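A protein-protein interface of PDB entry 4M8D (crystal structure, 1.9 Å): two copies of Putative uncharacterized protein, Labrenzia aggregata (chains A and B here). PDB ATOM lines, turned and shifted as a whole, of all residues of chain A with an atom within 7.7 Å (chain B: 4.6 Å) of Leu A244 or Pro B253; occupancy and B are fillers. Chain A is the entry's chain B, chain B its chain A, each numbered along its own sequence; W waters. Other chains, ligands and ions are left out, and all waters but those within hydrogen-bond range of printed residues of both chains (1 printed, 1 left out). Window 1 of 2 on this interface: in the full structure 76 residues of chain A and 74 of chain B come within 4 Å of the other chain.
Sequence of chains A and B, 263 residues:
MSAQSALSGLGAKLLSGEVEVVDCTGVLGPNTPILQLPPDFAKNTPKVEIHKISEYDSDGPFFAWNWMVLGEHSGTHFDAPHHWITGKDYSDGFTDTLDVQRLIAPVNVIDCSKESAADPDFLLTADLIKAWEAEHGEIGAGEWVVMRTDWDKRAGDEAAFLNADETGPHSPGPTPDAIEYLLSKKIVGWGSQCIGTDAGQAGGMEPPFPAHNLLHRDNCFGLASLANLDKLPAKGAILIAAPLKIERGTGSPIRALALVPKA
O of Lys A245 is in hydrogen-bond range of N of Leu B28 (2.7 Å).
O of Leu B28 is in hydrogen-bond range of N of Glu A247.
O of Leu B70 is in hydrogen-bond range of N of Met A68 (2.7 Å).
The guanidinium group of Arg A255 sits at hydrogen-bond distance from the backbone carbonyl oxygen of Pro B243 (2.9 Å).
O of Thr A95 sits at hydrogen-bond distance from NH1 of Arg B255, 3.0 Å away.
The backbone carbonyl oxygen (O) of Pro A243 is in hydrogen-bond range of the guanidinium group (NH1) of Arg B255 (3.0 Å).
The backbone carbonyl oxygen (O) of Thr B76 lies within hydrogen-bond range of the backbone NH (N) of Ile B254 (3.0 Å).
The backbone NH (N) of Leu B244 lies within hydrogen-bond range of the side-chain hydroxyl (OG) of Ser B252, 2.9 Å away.
The side-chain hydroxyl (OG1) of Thr A95 lies within hydrogen-bond range of the backbone carbonyl oxygen (O) of Ile A246, 2.9 Å away.
The backbone carbonyl oxygen (O) of Gly A249 is in hydrogen-bond range of the backbone NH (N) of Thr A95, at 2.9 Å.
N of Leu A244 is in hydrogen-bond range of OG of Ser A252 (3.0 Å).
Leu B70 touches Leu A70 (CD2 to CD2, 3.97 Å).
Arg B255 touches Ala A242.
CD2 of Leu A244 touches O of Pro B253, 3.6 Å away.
C of Ile B254 touches CD2 of Leu A244, at 3.7 Å.
NH1 of Arg B255 touches O of Leu A244 (3.8 Å).
Arg B255 touches Lys A245 (NH1 to CA, 3.6 Å).
O of Leu B28 touches CA of Ile A246, 3.3 Å away.
Pro A253 touches Leu B244 (O to CD2, 3.5 Å).
Ile A254 touches Leu B244 (N to CD2, 3.6 Å).
NH1 of Arg A255 touches O of Leu B244, 3.8 Å away.
Printed residues of chain B within 4 Å of Leu A244: Pro B253, Ile B254 and Arg B255.
Printed residues of chain A within 4 Å of Pro B253: Leu A244.
Of the printed residues of chain A, Ile B254 touches Leu A244 (3.7 Å).
Of the printed residues of chain A, Pro B243 touches Arg A255.
Of the printed residues of chain B, Leu A70 touches Leu B70 (3.97 Å).
Of the printed residues of chain B, Ile A246 touches Leu B28.
Of the printed residues of chain B, Glu A247 touches Leu B28.
The nearest printed residue of chain B that does not touch Leu A244 is Leu B28 (4.05 Å).
The nearest residue of chain A that does not touch Pro B253 is Met A68 (6.1 Å).
The nearest printed residue of chain B that does not touch Arg A255 is Ile B254 (7.2 Å).
Hydrophobic or aromatic side chains of chain B that line the printed part of chain A: Leu B28, Leu B70 and Leu B244.
Of the 23 printed residues of chain A, 12 touch a printed residue of chain B.
Printed residues of chain A that touch a printed residue of chain B: Met A68, Leu A70, Thr A95, Ala A242, Pro A243, Leu A244, Lys A245, Ile A246, Glu A247, Pro A253, Ile A254 and Arg A255.
Among the printed residues, 16 pairs touch across the chains.
Leu B70 touches its own counterpart, Leu A70.
Pro A243 touches Arg B255, and with the chains exchanged Arg A255 touches Pro B243.
Leu A244 touches Pro B253, and with the chains exchanged Pro A253 touches Leu B244.
Leu A244 touches Arg B255, and with the chains exchanged Arg A255 touches Leu B244.
Positions printed for both chains: 28, 70, 243, 244, 252, 253, 254 and 255.
Water W1 bridges the backbone carbonyl oxygen of Ile B254 (2.8 Å) and the backbone NH of Lys A245 (3.0 Å).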
ATOM      1  N   LEU A  28      -3.098  26.663  29.056  1.00  0.00           N
ATOM      2  CA  LEU A  28      -2.022  27.398  28.419  1.00  0.00           C
ATOM      3  C   LEU A  28      -2.445  28.855  28.341  1.00  0.00           C
ATOM      4  O   LEU A  28      -3.395  29.186  27.637  1.00  0.00           O
ATOM      5  CB  LEU A  28      -1.739  26.814  27.030  1.00  0.00           C
ATOM      6  CG  LEU A  28      -0.662  27.460  26.146  1.00  0.00           C
ATOM      7  CD1 LEU A  28       0.699  27.396  26.819  1.00  0.00           C
ATOM      8  CD2 LEU A  28      -0.635  26.731  24.808  1.00  0.00           C
ATOM      9  N   MET A  68      -1.218  34.646  19.657  1.00  0.00           N
ATOM     10  CA  MET A  68      -0.359  34.335  20.783  1.00  0.00           C
ATOM     11  C   MET A  68       1.106  34.666  20.575  1.00  0.00           C
ATOM     12  O   MET A  68       1.634  34.564  19.466  1.00  0.00           O
ATOM     13  CB  MET A  68      -0.480  32.843  21.115  1.00  0.00           C
ATOM     14  CG  MET A  68      -1.870  32.433  21.571  1.00  0.00           C
ATOM     15  SD  MET A  68      -1.943  30.660  21.854  1.00  0.00           S
ATOM     16  CE  MET A  68      -0.879  30.509  23.287  1.00  0.00           C
ATOM     17  N   LEU A  70       4.048  32.654  21.801  1.00  0.00           N
ATOM     18  CA  LEU A  70       4.061  31.286  22.284  1.00  0.00           C
ATOM     19  C   LEU A  70       5.406  30.620  22.036  1.00  0.00           C
ATOM     20  O   LEU A  70       5.763  30.317  20.891  1.00  0.00           O
ATOM     21  CB  LEU A  70       2.940  30.475  21.615  1.00  0.00           C
ATOM     22  CG  LEU A  70       2.699  29.035  22.097  1.00  0.00           C
ATOM     23  CD1 LEU A  70       2.492  28.965  23.609  1.00  0.00           C
ATOM     24  CD2 LEU A  70       1.516  28.389  21.370  1.00  0.00           C
ATOM     25  N   PHE A  78       6.166  19.203  24.412  1.00  0.00           N
ATOM     26  CA  PHE A  78       6.881  18.072  23.821  1.00  0.00           C
ATOM     27  C   PHE A  78       8.281  18.544  23.470  1.00  0.00           C
ATOM     28  O   PHE A  78       8.431  19.636  22.927  1.00  0.00           O
ATOM     29  CB  PHE A  78       6.105  17.604  22.573  1.00  0.00           C
ATOM     30  CG  PHE A  78       6.727  16.457  21.794  1.00  0.00           C
ATOM     31  CD1 PHE A  78       7.768  16.680  20.897  1.00  0.00           C
ATOM     32  CD2 PHE A  78       6.177  15.176  21.871  1.00  0.00           C
ATOM     33  CE1 PHE A  78       8.310  15.628  20.135  1.00  0.00           C
ATOM     34  CE2 PHE A  78       6.690  14.132  21.117  1.00  0.00           C
ATOM     35  CZ  PHE A  78       7.755  14.353  20.232  1.00  0.00           C
ATOM     36  N   PHE A  94      13.126  16.858  14.236  1.00  0.00           N
ATOM     37  CA  PHE A  94      12.309  18.071  14.383  1.00  0.00           C
ATOM     38  C   PHE A  94      10.837  17.706  14.459  1.00  0.00           C
ATOM     39  O   PHE A  94      10.449  16.614  14.032  1.00  0.00           O
ATOM     40  CB  PHE A  94      12.519  19.038  13.216  1.00  0.00           C
ATOM     41  CG  PHE A  94      13.954  19.472  13.020  1.00  0.00           C
ATOM     42  CD1 PHE A  94      14.831  18.697  12.272  1.00  0.00           C
ATOM     43  CD2 PHE A  94      14.419  20.663  13.570  1.00  0.00           C
ATOM     44  CE1 PHE A  94      16.160  19.105  12.079  1.00  0.00           C
ATOM     45  CE2 PHE A  94      15.726  21.073  13.382  1.00  0.00           C
ATOM     46  CZ  PHE A  94      16.597  20.289  12.629  1.00  0.00           C
ATOM     47  N   THR A  95      10.018  18.631  14.959  1.00  0.00           N
ATOM     48  CA  THR A  95       8.583  18.389  15.085  1.00  0.00           C
ATOM     49  C   THR A  95       7.938  18.159  13.727  1.00  0.00           C
ATOM     50  O   THR A  95       6.929  17.492  13.663  1.00  0.00           O
ATOM     51  CB  THR A  95       7.845  19.556  15.787  1.00  0.00           C
ATOM     52  OG1 THR A  95       8.236  20.794  15.173  1.00  0.00           O
ATOM     53  CG2 THR A  95       8.187  19.585  17.311  1.00  0.00           C
ATOM     54  N   ASP A  96       8.525  18.690  12.654  1.00  0.00           N
ATOM     55  CA  ASP A  96       7.981  18.468  11.305  1.00  0.00           C
ATOM     56  C   ASP A  96       8.652  17.318  10.533  1.00  0.00           C
ATOM     57  O   ASP A  96       8.276  17.029   9.396  1.00  0.00           O
ATOM     58  CB  ASP A  96       8.067  19.759  10.472  1.00  0.00           C
ATOM     59  CG  ASP A  96       9.492  20.277  10.329  1.00  0.00           C
ATOM     60  OD1 ASP A  96      10.355  19.907  11.150  1.00  0.00           O
ATOM     61  OD2 ASP A  96       9.744  21.073   9.405  1.00  0.00           O
ATOM     62  N   THR A  97       9.648  16.666  11.121  1.00  0.00           N
ATOM     63  CA  THR A  97      10.308  15.572  10.416  1.00  0.00           C
ATOM     64  C   THR A  97      10.289  14.267  11.207  1.00  0.00           C
ATOM     65  O   THR A  97      10.631  13.217  10.667  1.00  0.00           O
ATOM     66  CB  THR A  97      11.764  15.920  10.061  1.00  0.00           C
ATOM     67  OG1 THR A  97      12.535  16.109  11.258  1.00  0.00           O
ATOM     68  CG2 THR A  97      11.801  17.181   9.221  1.00  0.00           C
ATOM     69  N   LEU A  98       9.859  14.317  12.469  1.00  0.00           N
ATOM     70  CA  LEU A  98       9.787  13.087  13.264  1.00  0.00           C
ATOM     71  C   LEU A  98       8.683  12.149  12.771  1.00  0.00           C
ATOM     72  O   LEU A  98       7.818  12.541  11.972  1.00  0.00           O
ATOM     73  CB  LEU A  98       9.599  13.407  14.747  1.00  0.00           C
ATOM     74  CG  LEU A  98       8.391  14.232  15.204  1.00  0.00           C
ATOM     75  CD1 LEU A  98       7.129  13.375  15.346  1.00  0.00           C
ATOM     76  CD2 LEU A  98       8.709  14.909  16.528  1.00  0.00           C
ATOM     77  N   ALA A 241       0.678  12.037  22.484  1.00  0.00           N
ATOM     78  CA  ALA A 241       1.420  13.251  22.754  1.00  0.00           C
ATOM     79  C   ALA A 241       2.067  13.718  21.460  1.00  0.00           C
ATOM     80  O   ALA A 241       3.141  13.247  21.103  1.00  0.00           O
ATOM     81  CB  ALA A 241       2.481  13.001  23.849  1.00  0.00           C
ATOM     82  N   ALA A 242       1.404  14.642  20.769  1.00  0.00           N
ATOM     83  CA  ALA A 242       1.771  15.009  19.405  1.00  0.00           C
ATOM     84  C   ALA A 242       2.080  16.497  19.292  1.00  0.00           C
ATOM     85  O   ALA A 242       1.225  17.335  19.577  1.00  0.00           O
ATOM     86  CB  ALA A 242       0.646  14.622  18.439  1.00  0.00           C
ATOM     87  N   PRO A 243       3.311  16.839  18.886  1.00  0.00           N
ATOM     88  CA  PRO A 243       3.640  18.254  18.728  1.00  0.00           C
ATOM     89  C   PRO A 243       3.025  18.850  17.464  1.00  0.00           C
ATOM     90  O   PRO A 243       2.803  18.127  16.491  1.00  0.00           O
ATOM     91  CB  PRO A 243       5.162  18.241  18.604  1.00  0.00           C
ATOM     92  CG  PRO A 243       5.446  16.940  17.913  1.00  0.00           C
ATOM     93  CD  PRO A 243       4.437  15.965  18.488  1.00  0.00           C
ATOM     94  N   LEU A 244       2.778  20.156  17.487  1.00  0.00           N
ATOM     95  CA  LEU A 244       2.452  20.914  16.289  1.00  0.00           C
ATOM     96  C   LEU A 244       3.536  20.682  15.246  1.00  0.00           C
ATOM     97  O   LEU A 244       4.697  20.446  15.600  1.00  0.00           O
ATOM     98  CB  LEU A 244       2.341  22.410  16.608  1.00  0.00           C
ATOM     99  CG  LEU A 244       1.288  22.816  17.653  1.00  0.00           C
ATOM    100  CD1 LEU A 244       1.247  24.327  17.836  1.00  0.00           C
ATOM    101  CD2 LEU A 244      -0.100  22.314  17.272  1.00  0.00           C
ATOM    102  N   LYS A 245       3.175  20.755  13.971  1.00  0.00           N
ATOM    103  CA  LYS A 245       4.149  20.470  12.917  1.00  0.00           C
ATOM    104  C   LYS A 245       4.947  21.739  12.596  1.00  0.00           C
ATOM    105  O   LYS A 245       4.998  22.195  11.466  1.00  0.00           O
ATOM    106  CB  LYS A 245       3.442  19.912  11.688  1.00  0.00           C
ATOM    107  CG  LYS A 245       4.371  19.194  10.703  1.00  0.00           C
ATOM    108  CD  LYS A 245       3.573  18.575   9.569  1.00  0.00           C
ATOM    109  CE  LYS A 245       4.469  17.657   8.722  1.00  0.00           C
ATOM    110  NZ  LYS A 245       3.637  16.819   7.796  1.00  0.00           N
ATOM    111  N   ILE A 246       5.556  22.316  13.632  1.00  0.00           N
ATOM    112  CA  ILE A 246       6.341  23.540  13.507  1.00  0.00           C
ATOM    113  C   ILE A 246       7.536  23.277  12.590  1.00  0.00           C
ATOM    114  O   ILE A 246       8.201  22.257  12.720  1.00  0.00           O
ATOM    115  CB  ILE A 246       6.800  24.019  14.896  1.00  0.00           C
ATOM    116  CG1 ILE A 246       5.571  24.354  15.763  1.00  0.00           C
ATOM    117  CG2 ILE A 246       7.744  25.234  14.804  1.00  0.00           C
ATOM    118  CD1 ILE A 246       5.910  24.531  17.237  1.00  0.00           C
ATOM    119  N   GLU A 247       7.769  24.175  11.640  1.00  0.00           N
ATOM    120  CA  GLU A 247       8.862  24.030  10.687  1.00  0.00           C
ATOM    121  C   GLU A 247      10.191  24.076  11.415  1.00  0.00           C
ATOM    122  O   GLU A 247      10.481  25.053  12.095  1.00  0.00           O
ATOM    123  CB  GLU A 247       8.824  25.133   9.636  1.00  0.00           C
ATOM    124  CG  GLU A 247       9.780  24.897   8.477  1.00  0.00           C
ATOM    125  CD  GLU A 247       9.479  25.807   7.305  1.00  0.00           C
ATOM    126  OE1 GLU A 247       9.270  27.008   7.542  1.00  0.00           O
ATOM    127  OE2 GLU A 247       9.426  25.319   6.149  1.00  0.00           O
ATOM    128  N   GLY A 249      10.852  22.652  14.051  1.00  0.00           N
ATOM    129  CA  GLY A 249      10.561  22.909  15.459  1.00  0.00           C
ATOM    130  C   GLY A 249      11.359  22.018  16.392  1.00  0.00           C
ATOM    131  O   GLY A 249      11.591  20.845  16.073  1.00  0.00           O
ATOM    132  N   THR A 250      11.770  22.567  17.534  1.00  0.00           N
ATOM    133  CA  THR A 250      12.532  21.808  18.543  1.00  0.00           C
ATOM    134  C   THR A 250      11.611  21.202  19.577  1.00  0.00           C
ATOM    135  O   THR A 250      12.011  20.358  20.371  1.00  0.00           O
ATOM    136  CB  THR A 250      13.565  22.681  19.294  1.00  0.00           C
ATOM    137  OG1 THR A 250      12.884  23.557  20.210  1.00  0.00           O
ATOM    138  CG2 THR A 250      14.394  23.488  18.307  1.00  0.00           C
ATOM    139  N   GLY A 251      10.364  21.639  19.565  1.00  0.00           N
ATOM    140  CA  GLY A 251       9.393  21.110  20.490  1.00  0.00           C
ATOM    141  C   GLY A 251       8.111  21.888  20.282  1.00  0.00           C
ATOM    142  O   GLY A 251       8.037  22.705  19.372  1.00  0.00           O
ATOM    143  N   SER A 252       7.130  21.676  21.149  1.00  0.00           N
ATOM    144  CA  SER A 252       5.829  22.267  20.939  1.00  0.00           C
ATOM    145  C   SER A 252       4.944  22.090  22.149  1.00  0.00           C
ATOM    146  O   SER A 252       4.986  21.054  22.799  1.00  0.00           O
ATOM    147  CB  SER A 252       5.162  21.617  19.708  1.00  0.00           C
ATOM    148  OG  SER A 252       3.816  21.997  19.599  1.00  0.00           O
ATOM    149  N   PRO A 253       4.106  23.093  22.435  1.00  0.00           N
ATOM    150  CA  PRO A 253       2.968  22.782  23.304  1.00  0.00           C
ATOM    151  C   PRO A 253       2.132  21.686  22.670  1.00  0.00           C
ATOM    152  O   PRO A 253       2.123  21.540  21.436  1.00  0.00           O
ATOM    153  CB  PRO A 253       2.188  24.099  23.371  1.00  0.00           C
ATOM    154  CG  PRO A 253       2.611  24.841  22.131  1.00  0.00           C
ATOM    155  CD  PRO A 253       4.020  24.437  21.837  1.00  0.00           C
ATOM    156  N   ILE A 254       1.428  20.924  23.506  1.00  0.00           N
ATOM    157  CA  ILE A 254       0.628  19.799  23.041  1.00  0.00           C
ATOM    158  C   ILE A 254      -0.670  19.703  23.833  1.00  0.00           C
ATOM    159  O   ILE A 254      -0.775  20.214  24.962  1.00  0.00           O
ATOM    160  CB  ILE A 254       1.382  18.455  23.194  1.00  0.00           C
ATOM    161  CG1 ILE A 254       1.729  18.203  24.678  1.00  0.00           C
ATOM    162  CG2 ILE A 254       2.651  18.432  22.341  1.00  0.00           C
ATOM    163  CD1 ILE A 254       2.335  16.776  24.914  1.00  0.00           C
ATOM    164  N   ARG A 255      -1.653  19.045  23.251  1.00  0.00           N
ATOM    165  CA  ARG A 255      -2.794  18.591  24.031  1.00  0.00           C
ATOM    166  C   ARG A 255      -2.540  17.114  24.316  1.00  0.00           C
ATOM    167  O   ARG A 255      -2.874  16.241  23.517  1.00  0.00           O
ATOM    168  CB  ARG A 255      -4.121  18.799  23.288  1.00  0.00           C
ATOM    169  CG  ARG A 255      -5.345  18.576  24.209  1.00  0.00           C
ATOM    170  CD  ARG A 255      -5.362  19.643  25.277  1.00  0.00           C
ATOM    171  NE  ARG A 255      -6.529  19.641  26.163  1.00  0.00           N
ATOM    172  CZ  ARG A 255      -7.599  20.418  26.021  1.00  0.00           C
ATOM    173  NH1 ARG A 255      -7.716  21.225  24.972  1.00  0.00           N
ATOM    174  NH2 ARG A 255      -8.565  20.380  26.935  1.00  0.00           N
ATOM    175  N   LEU B  28       3.705  24.003   9.896  1.00  0.00           N
ATOM    176  CA  LEU B  28       3.358  25.271  10.523  1.00  0.00           C
ATOM    177  C   LEU B  28       4.576  26.188  10.572  1.00  0.00           C
ATOM    178  O   LEU B  28       5.552  25.906  11.289  1.00  0.00           O
ATOM    179  CB  LEU B  28       2.790  25.035  11.927  1.00  0.00           C
ATOM    180  CG  LEU B  28       2.355  26.264  12.734  1.00  0.00           C
ATOM    181  CD1 LEU B  28       1.227  27.024  12.024  1.00  0.00           C
ATOM    182  CD2 LEU B  28       1.909  25.841  14.142  1.00  0.00           C
ATOM    183  N   LEU B  70       1.797  33.481  16.752  1.00  0.00           N
ATOM    184  CA  LEU B  70       0.922  32.389  16.327  1.00  0.00           C
ATOM    185  C   LEU B  70      -0.552  32.698  16.627  1.00  0.00           C
ATOM    186  O   LEU B  70      -0.964  32.704  17.787  1.00  0.00           O
ATOM    187  CB  LEU B  70       1.346  31.078  17.027  1.00  0.00           C
ATOM    188  CG  LEU B  70       0.694  29.754  16.634  1.00  0.00           C
ATOM    189  CD1 LEU B  70       0.768  29.516  15.131  1.00  0.00           C
ATOM    190  CD2 LEU B  70       1.306  28.575  17.409  1.00  0.00           C
ATOM    191  N   GLY B  71      -1.338  32.949  15.584  1.00  0.00           N
ATOM    192  CA  GLY B  71      -2.777  33.057  15.748  1.00  0.00           C
ATOM    193  C   GLY B  71      -3.359  31.706  16.105  1.00  0.00           C
ATOM    194  O   GLY B  71      -2.853  30.657  15.670  1.00  0.00           O
ATOM    195  N   GLU B  72      -4.436  31.717  16.884  1.00  0.00           N
ATOM    196  CA  GLU B  72      -5.185  30.494  17.140  1.00  0.00           C
ATOM    197  C   GLU B  72      -5.554  29.816  15.825  1.00  0.00           C
ATOM    198  O   GLU B  72      -5.471  28.592  15.702  1.00  0.00           O
ATOM    199  CB  GLU B  72      -6.463  30.796  17.927  1.00  0.00           C
ATOM    200  CG  GLU B  72      -6.264  31.285  19.350  1.00  0.00           C
ATOM    201  CD  GLU B  72      -7.578  31.774  19.949  1.00  0.00           C
ATOM    202  OE1 GLU B  72      -8.425  32.290  19.188  1.00  0.00           O
ATOM    203  OE2 GLU B  72      -7.778  31.631  21.170  1.00  0.00           O
ATOM    204  N   SER B  74      -4.455  29.185  12.680  1.00  0.00           N
ATOM    205  CA  SER B  74      -3.244  29.126  11.854  1.00  0.00           C
ATOM    206  C   SER B  74      -2.956  27.713  11.392  1.00  0.00           C
ATOM    207  O   SER B  74      -2.740  26.832  12.223  1.00  0.00           O
ATOM    208  CB  SER B  74      -2.013  29.631  12.632  1.00  0.00           C
ATOM    209  OG  SER B  74      -2.163  30.949  13.085  1.00  0.00           O
ATOM    210  N   THR B  76      -3.217  23.926   9.861  1.00  0.00           N
ATOM    211  CA  THR B  76      -4.144  22.883  10.276  1.00  0.00           C
ATOM    212  C   THR B  76      -4.612  23.250  11.668  1.00  0.00           C
ATOM    213  O   THR B  76      -3.793  23.350  12.591  1.00  0.00           O
ATOM    214  CB  THR B  76      -3.483  21.496  10.282  1.00  0.00           C
ATOM    215  OG1 THR B  76      -2.875  21.267   9.009  1.00  0.00           O
ATOM    216  CG2 THR B  76      -4.524  20.399  10.550  1.00  0.00           C
ATOM    217  N   HIS B  77      -5.906  23.511  11.823  1.00  0.00           N
ATOM    218  CA  HIS B  77      -6.357  24.068  13.084  1.00  0.00           C
ATOM    219  C   HIS B  77      -7.807  23.737  13.397  1.00  0.00           C
ATOM    220  O   HIS B  77      -8.554  23.233  12.550  1.00  0.00           O
ATOM    221  CB  HIS B  77      -6.096  25.604  13.127  1.00  0.00           C
ATOM    222  CG  HIS B  77      -7.098  26.455  12.384  1.00  0.00           C
ATOM    223  ND1 HIS B  77      -6.916  26.852  11.074  1.00  0.00           N
ATOM    224  CD2 HIS B  77      -8.254  27.041  12.796  1.00  0.00           C
ATOM    225  CE1 HIS B  77      -7.924  27.627  10.704  1.00  0.00           C
ATOM    226  NE2 HIS B  77      -8.759  27.737  11.722  1.00  0.00           N
ATOM    227  N   PRO B 243      -7.342  20.570  20.158  1.00  0.00           N
ATOM    228  CA  PRO B 243      -6.758  21.900  20.298  1.00  0.00           C
ATOM    229  C   PRO B 243      -5.864  21.976  21.526  1.00  0.00           C
ATOM    230  O   PRO B 243      -6.143  21.288  22.507  1.00  0.00           O
ATOM    231  CB  PRO B 243      -7.984  22.796  20.465  1.00  0.00           C
ATOM    232  CG  PRO B 243      -8.956  21.922  21.192  1.00  0.00           C
ATOM    233  CD  PRO B 243      -8.773  20.552  20.529  1.00  0.00           C
ATOM    234  N   LEU B 244      -4.816  22.790  21.463  1.00  0.00           N
ATOM    235  CA  LEU B 244      -4.081  23.203  22.666  1.00  0.00           C
ATOM    236  C   LEU B 244      -5.070  23.739  23.717  1.00  0.00           C
ATOM    237  O   LEU B 244      -6.105  24.280  23.359  1.00  0.00           O
ATOM    238  CB  LEU B 244      -3.056  24.280  22.326  1.00  0.00           C
ATOM    239  CG  LEU B 244      -2.011  23.894  21.280  1.00  0.00           C
ATOM    240  CD1 LEU B 244      -1.076  25.072  21.065  1.00  0.00           C
ATOM    241  CD2 LEU B 244      -1.230  22.631  21.713  1.00  0.00           C
ATOM    242  N   SER B 252      -7.392  26.653  17.838  1.00  0.00           N
ATOM    243  CA  SER B 252      -6.006  26.273  18.059  1.00  0.00           C
ATOM    244  C   SER B 252      -5.389  25.583  16.854  1.00  0.00           C
ATOM    245  O   SER B 252      -6.036  24.781  16.198  1.00  0.00           O
ATOM    246  CB  SER B 252      -5.913  25.340  19.271  1.00  0.00           C
ATOM    247  OG  SER B 252      -4.577  24.936  19.510  1.00  0.00           O
ATOM    248  N   PRO B 253      -4.112  25.880  16.578  1.00  0.00           N
ATOM    249  CA  PRO B 253      -3.374  24.970  15.702  1.00  0.00           C
ATOM    250  C   PRO B 253      -3.402  23.572  16.318  1.00  0.00           C
ATOM    251  O   PRO B 253      -3.455  23.469  17.559  1.00  0.00           O
ATOM    252  CB  PRO B 253      -1.940  25.537  15.690  1.00  0.00           C
ATOM    253  CG  PRO B 253      -2.015  26.882  16.380  1.00  0.00           C
ATOM    254  CD  PRO B 253      -3.261  26.907  17.212  1.00  0.00           C
ATOM    255  N   ILE B 254      -3.388  22.525  15.498  1.00  0.00           N
ATOM    256  CA  ILE B 254      -3.402  21.147  16.004  1.00  0.00           C
ATOM    257  C   ILE B 254      -2.433  20.270  15.244  1.00  0.00           C
ATOM    258  O   ILE B 254      -2.021  20.609  14.127  1.00  0.00           O
ATOM    259  CB  ILE B 254      -4.803  20.503  15.892  1.00  0.00           C
ATOM    260  CG1 ILE B 254      -5.252  20.470  14.415  1.00  0.00           C
ATOM    261  CG2 ILE B 254      -5.801  21.250  16.772  1.00  0.00           C
ATOM    262  CD1 ILE B 254      -6.635  19.899  14.214  1.00  0.00           C
ATOM    263  N   ARG B 255      -2.061  19.154  15.855  1.00  0.00           N
ATOM    264  CA  ARG B 255      -1.477  18.055  15.114  1.00  0.00           C
ATOM    265  C   ARG B 255      -2.589  17.057  14.890  1.00  0.00           C
ATOM    266  O   ARG B 255      -2.801  16.165  15.708  1.00  0.00           O
ATOM    267  CB  ARG B 255      -0.302  17.392  15.862  1.00  0.00           C
ATOM    268  CG  ARG B 255       0.532  16.439  14.962  1.00  0.00           C
ATOM    269  CD  ARG B 255       1.186  17.241  13.837  1.00  0.00           C
ATOM    270  NE  ARG B 255       2.061  16.484  12.915  1.00  0.00           N
ATOM    271  CZ  ARG B 255       3.391  16.443  13.006  1.00  0.00           C
ATOM    272  NH1 ARG B 255       4.010  17.034  14.021  1.00  0.00           N
ATOM    273  NH2 ARG B 255       4.107  15.796  12.089  1.00  0.00           N
HETATM  274  O   HOH W   1       0.428  21.905  13.632  1.00  0.00           O
